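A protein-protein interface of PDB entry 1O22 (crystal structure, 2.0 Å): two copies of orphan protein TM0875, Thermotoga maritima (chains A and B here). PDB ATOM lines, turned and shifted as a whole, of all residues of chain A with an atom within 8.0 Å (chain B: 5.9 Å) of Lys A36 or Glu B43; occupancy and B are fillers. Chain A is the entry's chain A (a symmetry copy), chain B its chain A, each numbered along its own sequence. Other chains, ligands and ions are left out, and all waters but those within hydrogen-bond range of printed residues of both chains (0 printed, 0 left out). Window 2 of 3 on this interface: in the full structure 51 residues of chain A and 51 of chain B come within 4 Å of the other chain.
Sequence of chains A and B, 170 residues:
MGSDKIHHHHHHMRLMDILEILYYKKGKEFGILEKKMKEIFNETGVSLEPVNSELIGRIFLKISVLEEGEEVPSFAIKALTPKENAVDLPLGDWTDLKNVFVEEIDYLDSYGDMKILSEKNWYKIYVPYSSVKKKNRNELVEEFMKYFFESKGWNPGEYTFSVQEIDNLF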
ATOM      1  N   LYS A  28      42.448 -24.209 -14.168  1.00  0.00           N
ATOM      2  CA  LYS A  28      41.127 -23.961 -14.735  1.00  0.00           C
ATOM      3  C   LYS A  28      40.711 -25.098 -15.670  1.00  0.00           C
ATOM      4  O   LYS A  28      41.498 -25.567 -16.504  1.00  0.00           O
ATOM      5  CB  LYS A  28      41.074 -22.616 -15.447  1.00  0.00           C
ATOM      6  CG  LYS A  28      39.633 -22.199 -15.736  1.00  0.00           C
ATOM      7  CD  LYS A  28      39.466 -20.737 -15.995  1.00  0.00           C
ATOM      8  CE  LYS A  28      38.050 -20.426 -16.465  1.00  0.00           C
ATOM      9  NZ  LYS A  28      37.040 -20.678 -15.414  1.00  0.00           N
ATOM     10  N   PHE A  30      38.140 -26.416 -18.570  1.00  0.00           N
ATOM     11  CA  PHE A  30      37.407 -25.856 -19.687  1.00  0.00           C
ATOM     12  C   PHE A  30      36.407 -26.799 -20.321  1.00  0.00           C
ATOM     13  O   PHE A  30      35.775 -26.444 -21.304  1.00  0.00           O
ATOM     14  CB  PHE A  30      38.383 -25.349 -20.733  1.00  0.00           C
ATOM     15  CG  PHE A  30      39.225 -24.226 -20.243  1.00  0.00           C
ATOM     16  CD1 PHE A  30      38.689 -22.961 -20.132  1.00  0.00           C
ATOM     17  CD2 PHE A  30      40.524 -24.442 -19.831  1.00  0.00           C
ATOM     18  CE1 PHE A  30      39.444 -21.911 -19.655  1.00  0.00           C
ATOM     19  CE2 PHE A  30      41.282 -23.391 -19.373  1.00  0.00           C
ATOM     20  CZ  PHE A  30      40.728 -22.122 -19.286  1.00  0.00           C
ATOM     21  N   GLY A  31      36.208 -27.966 -19.729  1.00  0.00           N
ATOM     22  CA  GLY A  31      35.349 -28.968 -20.316  1.00  0.00           C
ATOM     23  C   GLY A  31      33.901 -28.529 -20.400  1.00  0.00           C
ATOM     24  O   GLY A  31      33.251 -28.802 -21.404  1.00  0.00           O
ATOM     25  N   ILE A  32      33.376 -27.858 -19.368  1.00  0.00           N
ATOM     26  CA  ILE A  32      31.990 -27.419 -19.441  1.00  0.00           C
ATOM     27  C   ILE A  32      31.853 -26.219 -20.415  1.00  0.00           C
ATOM     28  O   ILE A  32      30.800 -26.056 -21.017  1.00  0.00           O
ATOM     29  CB  ILE A  32      31.363 -27.145 -18.035  1.00  0.00           C
ATOM     30  CG2 ILE A  32      31.355 -25.671 -17.679  1.00  0.00           C
ATOM     31  N   LEU A  33      32.903 -25.409 -20.563  1.00  0.00           N
ATOM     32  CA  LEU A  33      32.915 -24.308 -21.539  1.00  0.00           C
ATOM     33  C   LEU A  33      32.760 -24.909 -22.949  1.00  0.00           C
ATOM     34  O   LEU A  33      31.876 -24.518 -23.690  1.00  0.00           O
ATOM     35  CB  LEU A  33      34.227 -23.503 -21.466  1.00  0.00           C
ATOM     36  CG  LEU A  33      34.404 -22.356 -22.471  1.00  0.00           C
ATOM     37  CD1 LEU A  33      33.468 -21.231 -22.148  1.00  0.00           C
ATOM     38  CD2 LEU A  33      35.828 -21.841 -22.492  1.00  0.00           C
ATOM     39  N   GLU A  34      33.621 -25.875 -23.270  1.00  0.00           N
ATOM     40  CA  GLU A  34      33.634 -26.537 -24.566  1.00  0.00           C
ATOM     41  C   GLU A  34      32.304 -27.229 -24.874  1.00  0.00           C
ATOM     42  O   GLU A  34      31.857 -27.207 -26.030  1.00  0.00           O
ATOM     43  CB  GLU A  34      34.774 -27.536 -24.639  1.00  0.00           C
ATOM     44  CG  GLU A  34      36.142 -26.881 -24.588  1.00  0.00           C
ATOM     45  CD  GLU A  34      37.253 -27.842 -24.165  1.00  0.00           C
ATOM     46  OE1 GLU A  34      37.049 -29.082 -24.216  1.00  0.00           O
ATOM     47  OE2 GLU A  34      38.343 -27.348 -23.777  1.00  0.00           O
ATOM     48  N   LYS A  35      31.676 -27.817 -23.850  1.00  0.00           N
ATOM     49  CA  LYS A  35      30.393 -28.505 -24.030  1.00  0.00           C
ATOM     50  C   LYS A  35      29.302 -27.490 -24.328  1.00  0.00           C
ATOM     51  O   LYS A  35      28.481 -27.723 -25.203  1.00  0.00           O
ATOM     52  CB  LYS A  35      30.002 -29.372 -22.815  1.00  0.00           C
ATOM     53  CG  LYS A  35      28.575 -29.960 -22.936  1.00  0.00           C
ATOM     54  CD  LYS A  35      28.430 -31.381 -22.372  1.00  0.00           C
ATOM     55  CE  LYS A  35      27.265 -32.133 -23.070  1.00  0.00           C
ATOM     56  NZ  LYS A  35      27.290 -33.601 -22.845  1.00  0.00           N
ATOM     57  N   LYS A  36      29.311 -26.359 -23.617  1.00  0.00           N
ATOM     58  CA  LYS A  36      28.320 -25.307 -23.823  1.00  0.00           C
ATOM     59  C   LYS A  36      28.532 -24.582 -25.163  1.00  0.00           C
ATOM     60  O   LYS A  36      27.559 -24.206 -25.779  1.00  0.00           O
ATOM     61  CB  LYS A  36      28.276 -24.323 -22.635  1.00  0.00           C
ATOM     62  CG  LYS A  36      27.737 -24.998 -21.360  1.00  0.00           C
ATOM     63  CD  LYS A  36      27.266 -24.023 -20.280  1.00  0.00           C
ATOM     64  CE  LYS A  36      26.437 -24.767 -19.199  1.00  0.00           C
ATOM     65  NZ  LYS A  36      25.548 -23.849 -18.430  1.00  0.00           N
ATOM     66  N   MET A  37      29.770 -24.456 -25.636  1.00  0.00           N
ATOM     67  CA  MET A  37      30.050 -23.853 -26.950  1.00  0.00           C
ATOM     68  C   MET A  37      29.481 -24.722 -28.040  1.00  0.00           C
ATOM     69  O   MET A  37      28.879 -24.224 -28.980  1.00  0.00           O
ATOM     70  CB  MET A  37      31.554 -23.731 -27.187  1.00  0.00           C
ATOM     71  CG  MET A  37      32.227 -22.638 -26.374  1.00  0.00           C
ATOM     72  SD  MET A  37      34.205 -22.693 -26.552  1.00  0.00           S
ATOM     73  CE  MET A  37      34.279 -23.148 -28.434  1.00  0.00           C
ATOM     74  N   LYS A  38      29.682 -26.039 -27.908  1.00  0.00           N
ATOM     75  CA  LYS A  38      29.139 -26.988 -28.857  1.00  0.00           C
ATOM     76  C   LYS A  38      27.593 -27.004 -28.844  1.00  0.00           C
ATOM     77  O   LYS A  38      26.969 -26.978 -29.896  1.00  0.00           O
ATOM     78  CB  LYS A  38      29.716 -28.388 -28.650  1.00  0.00           C
ATOM     79  CG  LYS A  38      29.192 -29.392 -29.700  1.00  0.00           C
ATOM     80  CD  LYS A  38      30.219 -30.497 -30.009  1.00  0.00           C
ATOM     81  CE  LYS A  38      31.363 -29.966 -30.874  1.00  0.00           C
ATOM     82  NZ  LYS A  38      30.918 -29.307 -32.144  1.00  0.00           N
ATOM     83  N   GLU A  39      26.991 -27.013 -27.662  1.00  0.00           N
ATOM     84  CA  GLU A  39      25.546 -26.871 -27.540  1.00  0.00           C
ATOM     85  C   GLU A  39      24.995 -25.605 -28.219  1.00  0.00           C
ATOM     86  O   GLU A  39      23.989 -25.671 -28.916  1.00  0.00           O
ATOM     87  CB  GLU A  39      25.145 -26.896 -26.062  1.00  0.00           C
ATOM     88  CG  GLU A  39      25.274 -28.288 -25.426  1.00  0.00           C
ATOM     89  CD  GLU A  39      25.109 -28.280 -23.907  1.00  0.00           C
ATOM     90  OE1 GLU A  39      25.410 -29.323 -23.276  1.00  0.00           O
ATOM     91  OE2 GLU A  39      24.683 -27.237 -23.341  1.00  0.00           O
ATOM     92  N   ILE A  40      25.643 -24.455 -28.001  1.00  0.00           N
ATOM     93  CA  ILE A  40      25.213 -23.191 -28.624  1.00  0.00           C
ATOM     94  C   ILE A  40      25.338 -23.241 -30.138  1.00  0.00           C
ATOM     95  O   ILE A  40      24.462 -22.768 -30.830  1.00  0.00           O
ATOM     96  CB  ILE A  40      26.003 -22.000 -28.070  1.00  0.00           C
ATOM     97  CG1 ILE A  40      25.671 -21.784 -26.583  1.00  0.00           C
ATOM     98  CG2 ILE A  40      25.698 -20.721 -28.869  1.00  0.00           C
ATOM     99  CD1 ILE A  40      26.580 -20.789 -25.897  1.00  0.00           C
ATOM    100  N   PHE A  41      26.423 -23.818 -30.649  1.00  0.00           N
ATOM    101  CA  PHE A  41      26.607 -24.045 -32.089  1.00  0.00           C
ATOM    102  C   PHE A  41      25.547 -24.916 -32.705  1.00  0.00           C
ATOM    103  O   PHE A  41      25.084 -24.633 -33.826  1.00  0.00           O
ATOM    104  CB  PHE A  41      27.990 -24.633 -32.391  1.00  0.00           C
ATOM    105  CG  PHE A  41      28.227 -24.894 -33.851  1.00  0.00           C
ATOM    106  CD1 PHE A  41      28.280 -23.838 -34.761  1.00  0.00           C
ATOM    107  CD2 PHE A  41      28.363 -26.184 -34.324  1.00  0.00           C
ATOM    108  CE1 PHE A  41      28.495 -24.069 -36.116  1.00  0.00           C
ATOM    109  CE2 PHE A  41      28.587 -26.422 -35.682  1.00  0.00           C
ATOM    110  CZ  PHE A  41      28.646 -25.368 -36.574  1.00  0.00           C
ATOM    111  N   ASN A  42      25.153 -25.976 -32.006  1.00  0.00           N
ATOM    112  CA  ASN A  42      24.164 -26.914 -32.542  1.00  0.00           C
ATOM    113  C   ASN A  42      22.734 -26.301 -32.556  1.00  0.00           C
ATOM    114  O   ASN A  42      21.897 -26.680 -33.355  1.00  0.00           O
ATOM    115  CB  ASN A  42      24.170 -28.231 -31.752  1.00  0.00           C
ATOM    116  CG  ASN A  42      25.435 -29.087 -31.999  1.00  0.00           C
ATOM    117  OD1 ASN A  42      26.136 -28.944 -33.002  1.00  0.00           O
ATOM    118  ND2 ASN A  42      25.701 -29.997 -31.079  1.00  0.00           N
ATOM    119  N   GLU A  43      22.486 -25.337 -31.678  1.00  0.00           N
ATOM    120  CA  GLU A  43      21.172 -24.694 -31.545  1.00  0.00           C
ATOM    121  C   GLU A  43      21.049 -23.440 -32.455  1.00  0.00           C
ATOM    122  O   GLU A  43      20.071 -23.294 -33.219  1.00  0.00           O
ATOM    123  CB  GLU A  43      20.976 -24.327 -30.071  1.00  0.00           C
ATOM    124  CG  GLU A  43      19.708 -23.565 -29.742  1.00  0.00           C
ATOM    125  CD  GLU A  43      19.466 -23.479 -28.241  1.00  0.00           C
ATOM    126  OE1 GLU A  43      20.429 -23.713 -27.459  1.00  0.00           O
ATOM    127  OE2 GLU A  43      18.312 -23.184 -27.846  1.00  0.00           O
ATOM    128  N   VAL A  46      25.908 -20.690 -34.495  1.00  0.00           N
ATOM    129  CA  VAL A  46      26.919 -19.665 -34.247  1.00  0.00           C
ATOM    130  C   VAL A  46      27.980 -20.276 -33.388  1.00  0.00           C
ATOM    131  O   VAL A  46      27.688 -20.821 -32.285  1.00  0.00           O
ATOM    132  CB  VAL A  46      26.324 -18.404 -33.527  1.00  0.00           C
ATOM    133  CG1 VAL A  46      27.410 -17.399 -33.180  1.00  0.00           C
ATOM    134  CG2 VAL A  46      25.312 -17.739 -34.397  1.00  0.00           C
ATOM    135  N   LEU A  48      31.096 -19.779 -31.035  1.00  0.00           N
ATOM    136  CA  LEU A  48      31.639 -18.805 -30.107  1.00  0.00           C
ATOM    137  C   LEU A  48      33.047 -19.235 -29.703  1.00  0.00           C
ATOM    138  O   LEU A  48      33.298 -20.422 -29.549  1.00  0.00           O
ATOM    139  CB  LEU A  48      30.754 -18.727 -28.887  1.00  0.00           C
ATOM    140  CG  LEU A  48      29.320 -18.274 -29.084  1.00  0.00           C
ATOM    141  CD1 LEU A  48      28.499 -18.445 -27.806  1.00  0.00           C
ATOM    142  CD2 LEU A  48      29.260 -16.836 -29.553  1.00  0.00           C
ATOM    143  N   LYS B  38      26.093 -14.533 -21.795  1.00  0.00           N
ATOM    144  CA  LYS B  38      26.114 -13.945 -20.472  1.00  0.00           C
ATOM    145  C   LYS B  38      26.089 -15.017 -19.359  1.00  0.00           C
ATOM    146  O   LYS B  38      26.861 -14.941 -18.413  1.00  0.00           O
ATOM    147  CB  LYS B  38      24.994 -12.921 -20.290  1.00  0.00           C
ATOM    148  CG  LYS B  38      25.050 -12.242 -18.904  1.00  0.00           C
ATOM    149  CD  LYS B  38      24.508 -10.801 -18.942  1.00  0.00           C
ATOM    150  CE  LYS B  38      25.503  -9.851 -19.610  1.00  0.00           C
ATOM    151  NZ  LYS B  38      26.872  -9.869 -19.003  1.00  0.00           N
ATOM    152  N   GLU B  39      25.230 -16.021 -19.494  1.00  0.00           N
ATOM    153  CA  GLU B  39      25.236 -17.159 -18.585  1.00  0.00           C
ATOM    154  C   GLU B  39      26.602 -17.860 -18.491  1.00  0.00           C
ATOM    155  O   GLU B  39      27.054 -18.179 -17.396  1.00  0.00           O
ATOM    156  CB  GLU B  39      24.155 -18.161 -19.001  1.00  0.00           C
ATOM    157  CG  GLU B  39      22.730 -17.666 -18.709  1.00  0.00           C
ATOM    158  CD  GLU B  39      21.643 -18.541 -19.330  1.00  0.00           C
ATOM    159  OE1 GLU B  39      20.466 -18.105 -19.333  1.00  0.00           O
ATOM    160  OE2 GLU B  39      21.959 -19.660 -19.819  1.00  0.00           O
ATOM    161  N   ILE B  40      27.247 -18.115 -19.634  1.00  0.00           N
ATOM    162  CA  ILE B  40      28.572 -18.759 -19.653  1.00  0.00           C
ATOM    163  C   ILE B  40      29.626 -17.892 -18.984  1.00  0.00           C
ATOM    164  O   ILE B  40      30.449 -18.402 -18.254  1.00  0.00           O
ATOM    165  CB  ILE B  40      29.004 -19.104 -21.083  1.00  0.00           C
ATOM    166  CG1 ILE B  40      28.083 -20.187 -21.672  1.00  0.00           C
ATOM    167  CG2 ILE B  40      30.466 -19.581 -21.113  1.00  0.00           C
ATOM    168  CD1 ILE B  40      28.285 -20.413 -23.154  1.00  0.00           C
ATOM    169  N   PHE B  41      29.596 -16.585 -19.229  1.00  0.00           N
ATOM    170  CA  PHE B  41      30.475 -15.622 -18.550  1.00  0.00           C
ATOM    171  C   PHE B  41      30.309 -15.600 -17.055  1.00  0.00           C
ATOM    172  O   PHE B  41      31.309 -15.510 -16.320  1.00  0.00           O
ATOM    173  CB  PHE B  41      30.288 -14.205 -19.105  1.00  0.00           C
ATOM    174  CG  PHE B  41      31.157 -13.179 -18.438  1.00  0.00           C
ATOM    175  CD1 PHE B  41      32.546 -13.236 -18.560  1.00  0.00           C
ATOM    176  CD2 PHE B  41      30.601 -12.179 -17.664  1.00  0.00           C
ATOM    177  CE1 PHE B  41      33.359 -12.292 -17.943  1.00  0.00           C
ATOM    178  CE2 PHE B  41      31.413 -11.224 -17.048  1.00  0.00           C
ATOM    179  CZ  PHE B  41      32.787 -11.285 -17.183  1.00  0.00           C
ATOM    180  N   ASN B  42      29.068 -15.672 -16.583  1.00  0.00           N
ATOM    181  CA  ASN B  42      28.798 -15.606 -15.145  1.00  0.00           C
ATOM    182  C   ASN B  42      29.229 -16.911 -14.415  1.00  0.00           C
ATOM    183  O   ASN B  42      29.538 -16.898 -13.238  1.00  0.00           O
ATOM    184  CB  ASN B  42      27.314 -15.313 -14.877  1.00  0.00           C
ATOM    185  CG  ASN B  42      26.901 -13.866 -15.241  1.00  0.00           C
ATOM    186  OD1 ASN B  42      27.725 -12.954 -15.329  1.00  0.00           O
ATOM    187  ND2 ASN B  42      25.609 -13.667 -15.424  1.00  0.00           N
ATOM    188  N   GLU B  43      29.267 -18.020 -15.143  1.00  0.00           N
ATOM    189  CA  GLU B  43      29.614 -19.334 -14.583  1.00  0.00           C
ATOM    190  C   GLU B  43      31.139 -19.617 -14.678  1.00  0.00           C
ATOM    191  O   GLU B  43      31.786 -19.991 -13.677  1.00  0.00           O
ATOM    192  CB  GLU B  43      28.808 -20.394 -15.339  1.00  0.00           C
ATOM    193  CG  GLU B  43      29.096 -21.834 -14.966  1.00  0.00           C
ATOM    194  CD  GLU B  43      28.076 -22.794 -15.563  1.00  0.00           C
ATOM    195  OE1 GLU B  43      27.355 -22.394 -16.518  1.00  0.00           O
ATOM    196  OE2 GLU B  43      27.993 -23.946 -15.072  1.00  0.00           O
ATOM    197  N   THR B  44      31.700 -19.399 -15.870  1.00  0.00           N
ATOM    198  CA  THR B  44      33.113 -19.708 -16.177  1.00  0.00           C
ATOM    199  C   THR B  44      34.079 -18.513 -16.076  1.00  0.00           C
ATOM    200  O   THR B  44      35.304 -18.683 -15.953  1.00  0.00           O
ATOM    201  CB  THR B  44      33.217 -20.360 -17.588  1.00  0.00           C
ATOM    202  OG1 THR B  44      32.951 -19.400 -18.621  1.00  0.00           O
ATOM    203  CG2 THR B  44      32.114 -21.430 -17.796  1.00  0.00           C
ATOM    204  N   GLY B  45      33.542 -17.303 -16.161  1.00  0.00           N
ATOM    205  CA  GLY B  45      34.370 -16.116 -16.190  1.00  0.00           C
ATOM    206  C   GLY B  45      34.985 -15.878 -17.564  1.00  0.00           C
ATOM    207  O   GLY B  45      35.849 -15.013 -17.719  1.00  0.00           O
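The side-chain amino group of Lys A36 is in salt-bridge range of the side-chain carboxylate of Glu B43 (3.0 Å). The backbone carbonyl oxygen (O) of Thr B44 sits at hydrogen-bond distance from the side-chain amino group (NZ) of Lys A28 (2.7 Å).
Of chain B, only Ile B40 (3.9 Å) and Glu B43 (3.0 Å) come within 4 Å of Lys A36. Glu B43 touches just one residue of chain A: Lys A36 (3.0 Å). Of the printed residues of chain B, Leu A33 touches Ile B40. Of the printed residues of chain B, Ile A40 touches Ile B40. Printed residues of chain A within 4 Å of Thr B44: Lys A28 (2.7 Å). The nearest residue of chain B that does not touch Lys A36 is Glu B39 (5.7 Å).
The backbone carbonyl oxygen (O) of Ile B40 lies within hydrogen-bond range of the side-chain hydroxyl (OG1) of Thr B44 (2.7 Å).
Ile A40 touches its own counterpart, Ile B40. Positions printed for both chains: 38, 39, 40, 41, 42 and 43. Of the 5 pairs that touch across the chains among the printed residues, 1 has its exchanged pair printed and touching as well.
Among the printed residues, merely in contact across the chains: Leu A33 with Ile B40 (3.6 Å), Lys A36 with Ile B40 (3.9 Å) and Ile A40 with Ile B40 (3.3 Å).
Of the 8 printed residues of chain B, 3 touch a printed residue of chain A. Hydrophobic or aromatic side chains of chain B within 4 Å of the printed part of chain A: Ile B40. Among the printed residues, Asp or Glu carboxylates within 4 Å of a Lys or Arg side-chain nitrogen of the other chain: Lys A36 with Glu B43 (3.0 Å).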
